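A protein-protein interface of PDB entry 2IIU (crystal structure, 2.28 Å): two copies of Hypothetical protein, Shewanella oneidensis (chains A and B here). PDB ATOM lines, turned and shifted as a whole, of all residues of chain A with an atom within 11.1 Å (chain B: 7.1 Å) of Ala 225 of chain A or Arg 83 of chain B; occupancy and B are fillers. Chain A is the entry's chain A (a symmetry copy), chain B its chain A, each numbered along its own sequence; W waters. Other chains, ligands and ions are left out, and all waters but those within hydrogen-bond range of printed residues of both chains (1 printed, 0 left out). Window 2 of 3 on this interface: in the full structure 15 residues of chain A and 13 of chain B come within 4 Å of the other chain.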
ATOM      1  N   PRO A  80     -35.213 -35.005   6.093  1.00  0.00           N
ATOM      2  CA  PRO A  80     -33.939 -34.478   5.576  1.00  0.00           C
ATOM      3  C   PRO A  80     -34.057 -33.446   4.434  1.00  0.00           C
ATOM      4  O   PRO A  80     -33.053 -32.875   4.041  1.00  0.00           O
ATOM      5  CB  PRO A  80     -33.265 -35.727   5.028  1.00  0.00           C
ATOM      6  CG  PRO A  80     -34.370 -36.552   4.575  1.00  0.00           C
ATOM      7  CD  PRO A  80     -35.449 -36.377   5.601  1.00  0.00           C
ATOM      8  N   VAL A  81     -35.263 -33.272   3.890  1.00  0.00           N
ATOM      9  CA  VAL A  81     -35.621 -32.327   2.802  1.00  0.00           C
ATOM     10  C   VAL A  81     -36.997 -31.681   3.117  1.00  0.00           C
ATOM     11  O   VAL A  81     -37.753 -32.221   3.890  1.00  0.00           O
ATOM     12  CB  VAL A  81     -35.724 -33.084   1.435  1.00  0.00           C
ATOM     13  CG1 VAL A  81     -34.388 -33.680   1.044  1.00  0.00           C
ATOM     14  CG2 VAL A  81     -36.772 -34.187   1.486  1.00  0.00           C
ATOM     15  N   GLU A  82     -37.319 -30.536   2.537  1.00  0.00           N
ATOM     16  CA  GLU A  82     -38.624 -29.901   2.754  1.00  0.00           C
ATOM     17  C   GLU A  82     -39.725 -30.572   1.961  1.00  0.00           C
ATOM     18  O   GLU A  82     -39.567 -30.873   0.776  1.00  0.00           O
ATOM     19  CB  GLU A  82     -38.611 -28.433   2.330  1.00  0.00           C
ATOM     20  CG  GLU A  82     -37.876 -27.550   3.246  1.00  0.00           C
ATOM     21  CD  GLU A  82     -38.715 -27.185   4.427  1.00  0.00           C
ATOM     22  OE1 GLU A  82     -39.920 -26.886   4.229  1.00  0.00           O
ATOM     23  OE2 GLU A  82     -38.168 -27.186   5.545  1.00  0.00           O
ATOM     24  N   ASP A  85     -40.585 -28.590  -1.113  1.00  0.00           N
ATOM     25  CA  ASP A  85     -39.676 -28.809  -2.223  1.00  0.00           C
ATOM     26  C   ASP A  85     -40.048 -30.078  -2.957  1.00  0.00           C
ATOM     27  O   ASP A  85     -40.071 -30.083  -4.186  1.00  0.00           O
ATOM     28  CB  ASP A  85     -38.213 -28.861  -1.749  1.00  0.00           C
ATOM     29  CG  ASP A  85     -37.681 -27.499  -1.405  1.00  0.00           C
ATOM     30  OD1 ASP A  85     -38.237 -26.528  -1.947  1.00  0.00           O
ATOM     31  OD2 ASP A  85     -36.769 -27.358  -0.557  1.00  0.00           O
ATOM     32  N   LEU A 143     -28.768 -38.114  -6.667  1.00  0.00           N
ATOM     33  CA  LEU A 143     -29.037 -37.390  -5.423  1.00  0.00           C
ATOM     34  C   LEU A 143     -29.073 -38.302  -4.207  1.00  0.00           C
ATOM     35  O   LEU A 143     -28.830 -37.840  -3.105  1.00  0.00           O
ATOM     36  CB  LEU A 143     -30.343 -36.601  -5.502  1.00  0.00           C
ATOM     37  CG  LEU A 143     -30.435 -35.469  -4.463  1.00  0.00           C
ATOM     38  CD1 LEU A 143     -29.246 -34.508  -4.594  1.00  0.00           C
ATOM     39  CD2 LEU A 143     -31.767 -34.705  -4.562  1.00  0.00           C
ATOM     40  N   LEU A 146     -25.777 -38.122  -2.678  1.00  0.00           N
ATOM     41  CA  LEU A 146     -25.549 -36.875  -1.950  1.00  0.00           C
ATOM     42  C   LEU A 146     -26.309 -36.872  -0.617  1.00  0.00           C
ATOM     43  O   LEU A 146     -25.906 -36.192   0.331  1.00  0.00           O
ATOM     44  CB  LEU A 146     -25.954 -35.681  -2.812  1.00  0.00           C
ATOM     45  CG  LEU A 146     -25.286 -34.370  -2.413  1.00  0.00           C
ATOM     46  CD1 LEU A 146     -23.770 -34.470  -2.542  1.00  0.00           C
ATOM     47  CD2 LEU A 146     -25.792 -33.266  -3.288  1.00  0.00           C
ATOM     48  N   ARG A 152     -21.056 -32.603   3.022  1.00  0.00           N
ATOM     49  CA  ARG A 152     -20.658 -31.220   3.259  1.00  0.00           C
ATOM     50  C   ARG A 152     -20.408 -30.474   1.938  1.00  0.00           C
ATOM     51  O   ARG A 152     -21.350 -30.035   1.273  1.00  0.00           O
ATOM     52  N   GLY A 153     -19.145 -30.365   1.534  1.00  0.00           N
ATOM     53  CA  GLY A 153     -18.789 -29.623   0.318  1.00  0.00           C
ATOM     54  C   GLY A 153     -19.234 -30.210  -1.011  1.00  0.00           C
ATOM     55  O   GLY A 153     -19.277 -29.495  -2.031  1.00  0.00           O
ATOM     56  N   ARG A 154     -19.596 -31.491  -1.010  1.00  0.00           N
ATOM     57  CA  ARG A 154     -19.971 -32.194  -2.251  1.00  0.00           C
ATOM     58  C   ARG A 154     -21.086 -31.560  -3.122  1.00  0.00           C
ATOM     59  O   ARG A 154     -21.097 -31.752  -4.332  1.00  0.00           O
ATOM     60  CB  ARG A 154     -20.306 -33.664  -1.926  1.00  0.00           C
ATOM     61  CG  ARG A 154     -19.088 -34.500  -1.488  1.00  0.00           C
ATOM     62  CD  ARG A 154     -19.449 -35.978  -1.292  1.00  0.00           C
ATOM     63  N   GLU A 155     -21.991 -30.799  -2.511  1.00  0.00           N
ATOM     64  CA  GLU A 155     -23.110 -30.170  -3.228  1.00  0.00           C
ATOM     65  C   GLU A 155     -22.711 -29.227  -4.379  1.00  0.00           C
ATOM     66  O   GLU A 155     -23.359 -29.217  -5.429  1.00  0.00           O
ATOM     67  CB  GLU A 155     -24.066 -29.473  -2.234  1.00  0.00           C
ATOM     68  CG  GLU A 155     -23.424 -28.454  -1.254  1.00  0.00           C
ATOM     69  CD  GLU A 155     -24.455 -27.484  -0.655  1.00  0.00           C
ATOM     70  N   VAL A 156     -21.633 -28.471  -4.202  1.00  0.00           N
ATOM     71  CA  VAL A 156     -21.140 -27.568  -5.240  1.00  0.00           C
ATOM     72  C   VAL A 156     -20.631 -28.348  -6.465  1.00  0.00           C
ATOM     73  O   VAL A 156     -20.913 -27.978  -7.614  1.00  0.00           O
ATOM     74  CB  VAL A 156     -20.052 -26.631  -4.671  1.00  0.00           C
ATOM     75  CG1 VAL A 156     -19.393 -25.799  -5.766  1.00  0.00           C
ATOM     76  CG2 VAL A 156     -20.677 -25.707  -3.627  1.00  0.00           C
ATOM     77  N   ASP A 157     -19.881 -29.424  -6.218  1.00  0.00           N
ATOM     78  CA  ASP A 157     -19.375 -30.260  -7.303  1.00  0.00           C
ATOM     79  C   ASP A 157     -20.547 -30.886  -8.073  1.00  0.00           C
ATOM     80  O   ASP A 157     -20.517 -30.957  -9.288  1.00  0.00           O
ATOM     81  CB  ASP A 157     -18.443 -31.359  -6.770  1.00  0.00           C
ATOM     82  CG  ASP A 157     -17.777 -32.171  -7.903  1.00  0.00           C
ATOM     83  N   PHE A 158     -21.571 -31.329  -7.349  1.00  0.00           N
ATOM     84  CA  PHE A 158     -22.783 -31.910  -7.930  1.00  0.00           C
ATOM     85  C   PHE A 158     -23.479 -30.941  -8.911  1.00  0.00           C
ATOM     86  O   PHE A 158     -23.831 -31.311 -10.035  1.00  0.00           O
ATOM     87  CB  PHE A 158     -23.747 -32.284  -6.791  1.00  0.00           C
ATOM     88  CG  PHE A 158     -25.005 -32.971  -7.240  1.00  0.00           C
ATOM     89  CD1 PHE A 158     -26.105 -32.247  -7.604  1.00  0.00           C
ATOM     90  CD2 PHE A 158     -25.082 -34.347  -7.274  1.00  0.00           C
ATOM     91  CE1 PHE A 158     -27.250 -32.868  -8.015  1.00  0.00           C
ATOM     92  CE2 PHE A 158     -26.228 -34.982  -7.681  1.00  0.00           C
ATOM     93  CZ  PHE A 158     -27.314 -34.232  -8.054  1.00  0.00           C
ATOM     94  N   VAL A 159     -23.689 -29.709  -8.455  1.00  0.00           N
ATOM     95  CA  VAL A 159     -24.304 -28.677  -9.261  1.00  0.00           C
ATOM     96  C   VAL A 159     -23.411 -28.308 -10.415  1.00  0.00           C
ATOM     97  O   VAL A 159     -23.901 -28.101 -11.533  1.00  0.00           O
ATOM     98  CB  VAL A 159     -24.653 -27.432  -8.402  1.00  0.00           C
ATOM     99  CG1 VAL A 159     -25.042 -26.235  -9.286  1.00  0.00           C
ATOM    100  CG2 VAL A 159     -25.748 -27.800  -7.437  1.00  0.00           C
ATOM    101  N   MET A 162     -23.843 -31.005 -13.036  1.00  0.00           N
ATOM    102  CA  MET A 162     -25.181 -30.873 -13.626  1.00  0.00           C
ATOM    103  C   MET A 162     -25.207 -29.760 -14.670  1.00  0.00           C
ATOM    104  O   MET A 162     -25.720 -29.934 -15.758  1.00  0.00           O
ATOM    105  CB  MET A 162     -26.189 -30.577 -12.526  1.00  0.00           C
ATOM    106  CG  MET A 162     -27.615 -30.666 -12.952  1.00  0.00           C
ATOM    107  SD  MET A 162     -28.832 -30.339 -11.420  1.00  0.00           S
ATOM    108  CE  MET A 162     -28.818 -28.300 -11.460  1.00  0.00           C
ATOM    109  N   GLY A 217     -34.038 -29.895 -12.652  1.00  0.00           N
ATOM    110  CA  GLY A 217     -32.698 -29.721 -12.075  1.00  0.00           C
ATOM    111  C   GLY A 217     -32.606 -28.437 -11.255  1.00  0.00           C
ATOM    112  O   GLY A 217     -31.880 -28.423 -10.251  1.00  0.00           O
ATOM    113  N   SER A 218     -33.343 -27.383 -11.660  1.00  0.00           N
ATOM    114  CA  SER A 218     -33.405 -26.148 -10.911  1.00  0.00           C
ATOM    115  C   SER A 218     -34.016 -26.357  -9.547  1.00  0.00           C
ATOM    116  O   SER A 218     -33.565 -25.745  -8.589  1.00  0.00           O
ATOM    117  CB  SER A 218     -34.210 -25.061 -11.642  1.00  0.00           C
ATOM    118  OG  SER A 218     -33.447 -24.636 -12.743  1.00  0.00           O
ATOM    119  N   ARG A 219     -35.100 -27.128  -9.479  1.00  0.00           N
ATOM    120  CA  ARG A 219     -35.686 -27.418  -8.180  1.00  0.00           C
ATOM    121  C   ARG A 219     -34.723 -28.178  -7.284  1.00  0.00           C
ATOM    122  O   ARG A 219     -34.655 -27.892  -6.096  1.00  0.00           O
ATOM    123  CB  ARG A 219     -37.015 -28.153  -8.267  1.00  0.00           C
ATOM    124  CG  ARG A 219     -37.611 -28.608  -6.852  1.00  0.00           C
ATOM    125  CD  ARG A 219     -37.886 -27.513  -5.795  1.00  0.00           C
ATOM    126  NE  ARG A 219     -38.575 -26.373  -6.417  1.00  0.00           N
ATOM    127  CZ  ARG A 219     -38.929 -25.262  -5.764  1.00  0.00           C
ATOM    128  NH1 ARG A 219     -38.717 -25.133  -4.456  1.00  0.00           N
ATOM    129  NH2 ARG A 219     -39.498 -24.269  -6.420  1.00  0.00           N
ATOM    130  N   LEU A 220     -33.951 -29.122  -7.836  1.00  0.00           N
ATOM    131  CA  LEU A 220     -32.955 -29.821  -7.026  1.00  0.00           C
ATOM    132  C   LEU A 220     -31.871 -28.903  -6.549  1.00  0.00           C
ATOM    133  O   LEU A 220     -31.362 -29.058  -5.414  1.00  0.00           O
ATOM    134  CB  LEU A 220     -32.238 -30.943  -7.767  1.00  0.00           C
ATOM    135  CG  LEU A 220     -32.870 -32.310  -7.866  1.00  0.00           C
ATOM    136  CD1 LEU A 220     -34.059 -32.273  -8.758  1.00  0.00           C
ATOM    137  CD2 LEU A 220     -31.802 -33.243  -8.426  1.00  0.00           C
ATOM    138  N   GLU A 221     -31.477 -27.971  -7.407  1.00  0.00           N
ATOM    139  CA  GLU A 221     -30.450 -27.027  -7.018  1.00  0.00           C
ATOM    140  C   GLU A 221     -30.955 -26.168  -5.852  1.00  0.00           C
ATOM    141  O   GLU A 221     -30.202 -25.915  -4.913  1.00  0.00           O
ATOM    142  CB  GLU A 221     -29.974 -26.218  -8.210  1.00  0.00           C
ATOM    143  CG  GLU A 221     -29.007 -25.107  -7.897  1.00  0.00           C
ATOM    144  CD  GLU A 221     -28.542 -24.397  -9.170  1.00  0.00           C
ATOM    145  OE1 GLU A 221     -29.146 -24.639 -10.228  1.00  0.00           O
ATOM    146  OE2 GLU A 221     -27.560 -23.644  -9.103  1.00  0.00           O
ATOM    147  N   LEU A 222     -32.221 -25.771  -5.871  1.00  0.00           N
ATOM    148  CA  LEU A 222     -32.786 -24.993  -4.756  1.00  0.00           C
ATOM    149  C   LEU A 222     -32.774 -25.750  -3.447  1.00  0.00           C
ATOM    150  O   LEU A 222     -32.506 -25.193  -2.382  1.00  0.00           O
ATOM    151  CB  LEU A 222     -34.226 -24.575  -5.034  1.00  0.00           C
ATOM    152  CG  LEU A 222     -34.397 -23.416  -6.015  1.00  0.00           C
ATOM    153  CD1 LEU A 222     -35.877 -23.205  -6.312  1.00  0.00           C
ATOM    154  CD2 LEU A 222     -33.775 -22.138  -5.499  1.00  0.00           C
ATOM    155  N   MET A 223     -33.064 -27.033  -3.521  1.00  0.00           N
ATOM    156  CA  MET A 223     -33.030 -27.879  -2.321  1.00  0.00           C
ATOM    157  C   MET A 223     -31.628 -27.961  -1.754  1.00  0.00           C
ATOM    158  O   MET A 223     -31.456 -27.879  -0.547  1.00  0.00           O
ATOM    159  CB  MET A 223     -33.503 -29.299  -2.618  1.00  0.00           C
ATOM    160  CG  MET A 223     -34.942 -29.359  -3.019  1.00  0.00           C
ATOM    161  SD  MET A 223     -35.548 -31.127  -3.652  1.00  0.00           S
ATOM    162  CE  MET A 223     -34.990 -32.029  -2.245  1.00  0.00           C
ATOM    163  N   LEU A 224     -30.626 -28.150  -2.614  1.00  0.00           N
ATOM    164  CA  LEU A 224     -29.256 -28.203  -2.148  1.00  0.00           C
ATOM    165  C   LEU A 224     -28.825 -26.875  -1.557  1.00  0.00           C
ATOM    166  O   LEU A 224     -27.973 -26.878  -0.677  1.00  0.00           O
ATOM    167  CB  LEU A 224     -28.289 -28.649  -3.261  1.00  0.00           C
ATOM    168  CG  LEU A 224     -28.583 -30.060  -3.784  1.00  0.00           C
ATOM    169  CD1 LEU A 224     -27.844 -30.419  -5.047  1.00  0.00           C
ATOM    170  CD2 LEU A 224     -28.270 -31.054  -2.696  1.00  0.00           C
ATOM    171  N   ALA A 225     -29.392 -25.756  -2.016  1.00  0.00           N
ATOM    172  CA  ALA A 225     -29.016 -24.452  -1.469  1.00  0.00           C
ATOM    173  C   ALA A 225     -29.541 -24.244  -0.077  1.00  0.00           C
ATOM    174  O   ALA A 225     -29.061 -23.352   0.607  1.00  0.00           O
ATOM    175  CB  ALA A 225     -29.477 -23.303  -2.386  1.00  0.00           C
ATOM    176  N   ARG A 226     -30.541 -25.020   0.363  1.00  0.00           N
ATOM    177  CA  ARG A 226     -31.056 -24.836   1.734  1.00  0.00           C
ATOM    178  C   ARG A 226     -30.139 -25.388   2.822  1.00  0.00           C
ATOM    179  O   ARG A 226     -30.429 -25.213   3.989  1.00  0.00           O
ATOM    180  CB  ARG A 226     -32.445 -25.417   1.940  1.00  0.00           C
ATOM    181  CG  ARG A 226     -33.465 -24.711   1.174  1.00  0.00           C
ATOM    182  CD  ARG A 226     -34.893 -25.160   1.533  1.00  0.00           C
ATOM    183  NE  ARG A 226     -35.723 -25.009   0.329  1.00  0.00           N
ATOM    184  CZ  ARG A 226     -36.386 -23.908  -0.011  1.00  0.00           C
ATOM    185  NH1 ARG A 226     -36.358 -22.844   0.774  1.00  0.00           N
ATOM    186  NH2 ARG A 226     -37.086 -23.873  -1.157  1.00  0.00           N
ATOM    187  N   VAL A 227     -29.049 -26.051   2.441  1.00  0.00           N
ATOM    188  CA  VAL A 227     -28.045 -26.595   3.386  1.00  0.00           C
ATOM    189  C   VAL A 227     -27.918 -28.126   3.311  1.00  0.00           C
ATOM    190  O   VAL A 227     -28.485 -28.779   2.426  1.00  0.00           O
ATOM    191  CB  VAL A 227     -28.317 -26.207   4.867  1.00  0.00           C
ATOM    192  N   THR B  72     -21.234 -20.242  -5.966  1.00  0.00           N
ATOM    193  CA  THR B  72     -20.594 -19.527  -4.844  1.00  0.00           C
ATOM    194  C   THR B  72     -21.539 -18.917  -3.804  1.00  0.00           C
ATOM    195  O   THR B  72     -22.771 -19.118  -3.808  1.00  0.00           O
ATOM    196  CB  THR B  72     -19.686 -18.362  -5.380  1.00  0.00           C
ATOM    197  OG1 THR B  72     -20.480 -17.434  -6.135  1.00  0.00           O
ATOM    198  CG2 THR B  72     -18.561 -18.887  -6.289  1.00  0.00           C
ATOM    199  N   GLY B  76     -23.944 -18.023   1.235  1.00  0.00           N
ATOM    200  CA  GLY B  76     -22.610 -18.379   1.711  1.00  0.00           C
ATOM    201  C   GLY B  76     -22.613 -18.873   3.147  1.00  0.00           C
ATOM    202  O   GLY B  76     -22.462 -20.069   3.386  1.00  0.00           O
ATOM    203  N   LEU B  77     -22.750 -17.951   4.103  1.00  0.00           N
ATOM    204  CA  LEU B  77     -22.807 -18.295   5.536  1.00  0.00           C
ATOM    205  C   LEU B  77     -23.813 -17.365   6.210  1.00  0.00           C
ATOM    206  O   LEU B  77     -25.030 -17.552   6.040  1.00  0.00           O
ATOM    207  CB  LEU B  77     -21.428 -18.207   6.200  1.00  0.00           C
ATOM    208  N   MET B  79     -26.167 -14.611   6.279  1.00  0.00           N
ATOM    209  CA  MET B  79     -26.869 -14.015   5.134  1.00  0.00           C
ATOM    210  C   MET B  79     -28.066 -13.114   5.463  1.00  0.00           C
ATOM    211  O   MET B  79     -28.994 -13.558   6.137  1.00  0.00           O
ATOM    212  CB  MET B  79     -27.415 -15.177   4.305  1.00  0.00           C
ATOM    213  CG  MET B  79     -26.398 -15.941   3.535  1.00  0.00           C
ATOM    214  SD  MET B  79     -26.042 -14.930   1.971  1.00  0.00           S
ATOM    215  CE  MET B  79     -27.621 -15.272   0.967  1.00  0.00           C
ATOM    216  N   VAL B  81     -30.312 -12.152   3.273  1.00  0.00           N
ATOM    217  CA  VAL B  81     -31.359 -12.612   2.326  1.00  0.00           C
ATOM    218  C   VAL B  81     -31.254 -14.150   2.152  1.00  0.00           C
ATOM    219  O   VAL B  81     -30.225 -14.718   2.429  1.00  0.00           O
ATOM    220  CB  VAL B  81     -31.163 -11.934   0.927  1.00  0.00           C
ATOM    221  CG1 VAL B  81     -31.323 -10.431   1.025  1.00  0.00           C
ATOM    222  CG2 VAL B  81     -29.799 -12.258   0.337  1.00  0.00           C
ATOM    223  N   GLU B  82     -32.305 -14.822   1.710  1.00  0.00           N
ATOM    224  CA  GLU B  82     -32.254 -16.270   1.475  1.00  0.00           C
ATOM    225  C   GLU B  82     -31.534 -16.616   0.190  1.00  0.00           C
ATOM    226  O   GLU B  82     -31.762 -16.004  -0.856  1.00  0.00           O
ATOM    227  CB  GLU B  82     -33.654 -16.871   1.369  1.00  0.00           C
ATOM    228  CG  GLU B  82     -34.365 -16.965   2.651  1.00  0.00           C
ATOM    229  CD  GLU B  82     -33.925 -18.167   3.422  1.00  0.00           C
ATOM    230  OE1 GLU B  82     -33.776 -19.249   2.799  1.00  0.00           O
ATOM    231  OE2 GLU B  82     -33.741 -18.032   4.646  1.00  0.00           O
ATOM    232  N   ARG B  83     -30.685 -17.630   0.289  1.00  0.00           N
ATOM    233  CA  ARG B  83     -29.965 -18.179  -0.833  1.00  0.00           C
ATOM    234  C   ARG B  83     -30.958 -18.581  -1.908  1.00  0.00           C
ATOM    235  O   ARG B  83     -30.729 -18.343  -3.069  1.00  0.00           O
ATOM    236  CB  ARG B  83     -29.179 -19.453  -0.392  1.00  0.00           C
ATOM    237  CG  ARG B  83     -27.809 -19.245   0.244  1.00  0.00           C
ATOM    238  CD  ARG B  83     -27.048 -20.593   0.603  1.00  0.00           C
ATOM    239  NE  ARG B  83     -27.406 -21.163   1.895  1.00  0.00           N
ATOM    240  N   THR B  84     -32.035 -19.236  -1.529  1.00  0.00           N
ATOM    241  CA  THR B  84     -32.986 -19.694  -2.536  1.00  0.00           C
ATOM    242  C   THR B  84     -33.689 -18.543  -3.237  1.00  0.00           C
ATOM    243  O   THR B  84     -33.900 -18.638  -4.403  1.00  0.00           O
ATOM    244  CB  THR B  84     -33.943 -20.682  -1.972  1.00  0.00           C
ATOM    245  OG1 THR B  84     -34.603 -20.094  -0.850  1.00  0.00           O
ATOM    246  CG2 THR B  84     -33.193 -21.979  -1.541  1.00  0.00           C
ATOM    247  N   ASP B  85     -33.970 -17.445  -2.547  1.00  0.00           N
ATOM    248  CA  ASP B  85     -34.536 -16.278  -3.199  1.00  0.00           C
ATOM    249  C   ASP B  85     -33.575 -15.745  -4.239  1.00  0.00           C
ATOM    250  O   ASP B  85     -33.999 -15.417  -5.345  1.00  0.00           O
ATOM    251  CB  ASP B  85     -34.898 -15.185  -2.179  1.00  0.00           C
ATOM    252  CG  ASP B  85     -36.141 -15.525  -1.404  1.00  0.00           C
ATOM    253  OD1 ASP B  85     -36.938 -16.313  -1.942  1.00  0.00           O
ATOM    254  OD2 ASP B  85     -36.316 -15.085  -0.244  1.00  0.00           O
ATOM    255  N   LEU B  86     -32.281 -15.710  -3.926  1.00  0.00           N
ATOM    256  CA  LEU B  86     -31.316 -15.172  -4.896  1.00  0.00           C
ATOM    257  C   LEU B  86     -31.250 -16.032  -6.099  1.00  0.00           C
ATOM    258  O   LEU B  86     -31.157 -15.525  -7.188  1.00  0.00           O
ATOM    259  CB  LEU B  86     -29.906 -14.972  -4.314  1.00  0.00           C
ATOM    260  CG  LEU B  86     -29.877 -14.006  -3.113  1.00  0.00           C
ATOM    261  CD1 LEU B  86     -28.556 -14.113  -2.338  1.00  0.00           C
ATOM    262  CD2 LEU B  86     -30.163 -12.584  -3.520  1.00  0.00           C
ATOM    263  N   LEU B  87     -31.310 -17.344  -5.908  1.00  0.00           N
ATOM    264  CA  LEU B  87     -31.295 -18.263  -7.052  1.00  0.00           C
ATOM    265  C   LEU B  87     -32.549 -18.103  -7.926  1.00  0.00           C
ATOM    266  O   LEU B  87     -32.449 -18.024  -9.147  1.00  0.00           O
ATOM    267  CB  LEU B  87     -31.160 -19.726  -6.582  1.00  0.00           C
ATOM    268  CG  LEU B  87     -29.799 -20.113  -6.008  1.00  0.00           C
ATOM    269  CD1 LEU B  87     -29.833 -21.554  -5.526  1.00  0.00           C
ATOM    270  CD2 LEU B  87     -28.698 -19.914  -7.050  1.00  0.00           C
ATOM    271  N   GLU B  88     -33.711 -18.021  -7.294  1.00  0.00           N
ATOM    272  CA  GLU B  88     -34.949 -17.817  -8.051  1.00  0.00           C
ATOM    273  C   GLU B  88     -34.942 -16.454  -8.783  1.00  0.00           C
ATOM    274  O   GLU B  88     -35.375 -16.372  -9.918  1.00  0.00           O
ATOM    275  CB  GLU B  88     -36.145 -17.969  -7.133  1.00  0.00           C
ATOM    276  CG  GLU B  88     -36.171 -19.380  -6.578  1.00  0.00           C
ATOM    277  CD  GLU B  88     -37.529 -19.851  -6.135  1.00  0.00           C
ATOM    278  OE1 GLU B  88     -38.301 -20.177  -7.044  1.00  0.00           O
ATOM    279  OE2 GLU B  88     -37.788 -19.972  -4.897  1.00  0.00           O
ATOM    280  N   LEU B  89     -34.395 -15.423  -8.148  1.00  0.00           N
ATOM    281  CA  LEU B  89     -34.280 -14.129  -8.770  1.00  0.00           C
ATOM    282  C   LEU B  89     -33.405 -14.255 -10.009  1.00  0.00           C
ATOM    283  O   LEU B  89     -33.785 -13.837 -11.096  1.00  0.00           O
ATOM    284  CB  LEU B  89     -33.700 -13.132  -7.750  1.00  0.00           C
ATOM    285  CG  LEU B  89     -33.465 -11.706  -8.238  1.00  0.00           C
ATOM    286  CD1 LEU B  89     -34.789 -11.098  -8.666  1.00  0.00           C
ATOM    287  CD2 LEU B  89     -32.807 -10.858  -7.128  1.00  0.00           C
HETATM  288  O   HOH W   1     -39.659 -22.257  -3.551  1.00  0.00           O
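NE of Arg 83 of chain B sits at hydrogen-bond distance from O of Ala 225 of chain A, 3.0 Å away.
NE of Arg 226 of chain A lies within salt-bridge range of OD2 of Asp 85 of chain A (2.7 Å).
Among the printed residues, merely in contact across the chains: Leu 222 of chain A with Thr 84 of chain B, Ala 225 of chain A with Leu 87 of chain B, Arg 226 of chain A with Thr 84 of chain B, Leu 222 of chain A with Leu 87 of chain B and Leu 222 of chain A with Glu 88 of chain B.
Ser 218 of chain A touches none of the printed residues of chain B. Of the printed residues of chain B, Leu 222 of chain A touches Thr 84 (3.4 Å), Leu 87 (3.7 Å) and Glu 88 (3.7 Å). Ala 225 of chain A touches just these residues of chain B: Arg 83 and Leu 87. Of the printed residues of chain B, Arg 226 of chain A touches Thr 84. Thr 72 of chain B touches none of the printed residues of chain A. No residue of chain A comes within 4 Å of Gly 76 of chain B. Glu 82 of chain B touches none of the printed residues of chain A. Of the printed residues of chain A, Arg 83 of chain B touches Ala 225. Of chain A, only Leu 222 and Arg 226 come within 4 Å of Thr 84 of chain B. Asp 85 of chain B touches none of the printed residues of chain A. Of chain A, only Leu 222 and Ala 225 come within 4 Å of Leu 87 of chain B. Of the printed residues of chain A, Glu 88 of chain B touches Leu 222 (3.7 Å). The nearest residue of chain B that does not touch Ala 225 of chain A is Thr 84 of chain B (4.03 Å).
Of the 13 printed residues of chain B, 4 touch a printed residue of chain A. Hydrophobic or aromatic side chains of chain B within 4 Å of the printed part of chain A: Leu 87. Among the printed residues, 6 pairs touch across the chains.
Positions printed for both chains: 81, 82 and 85. Of the 6 pairs that touch across the chains among the printed residues, none has its exchanged pair printed and touching as well.
Water W1 lies within hydrogen-bond range of NH1 of Arg 219 of chain A (3.2 Å) and OE2 of Glu 88 of chain B (3.2 Å).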
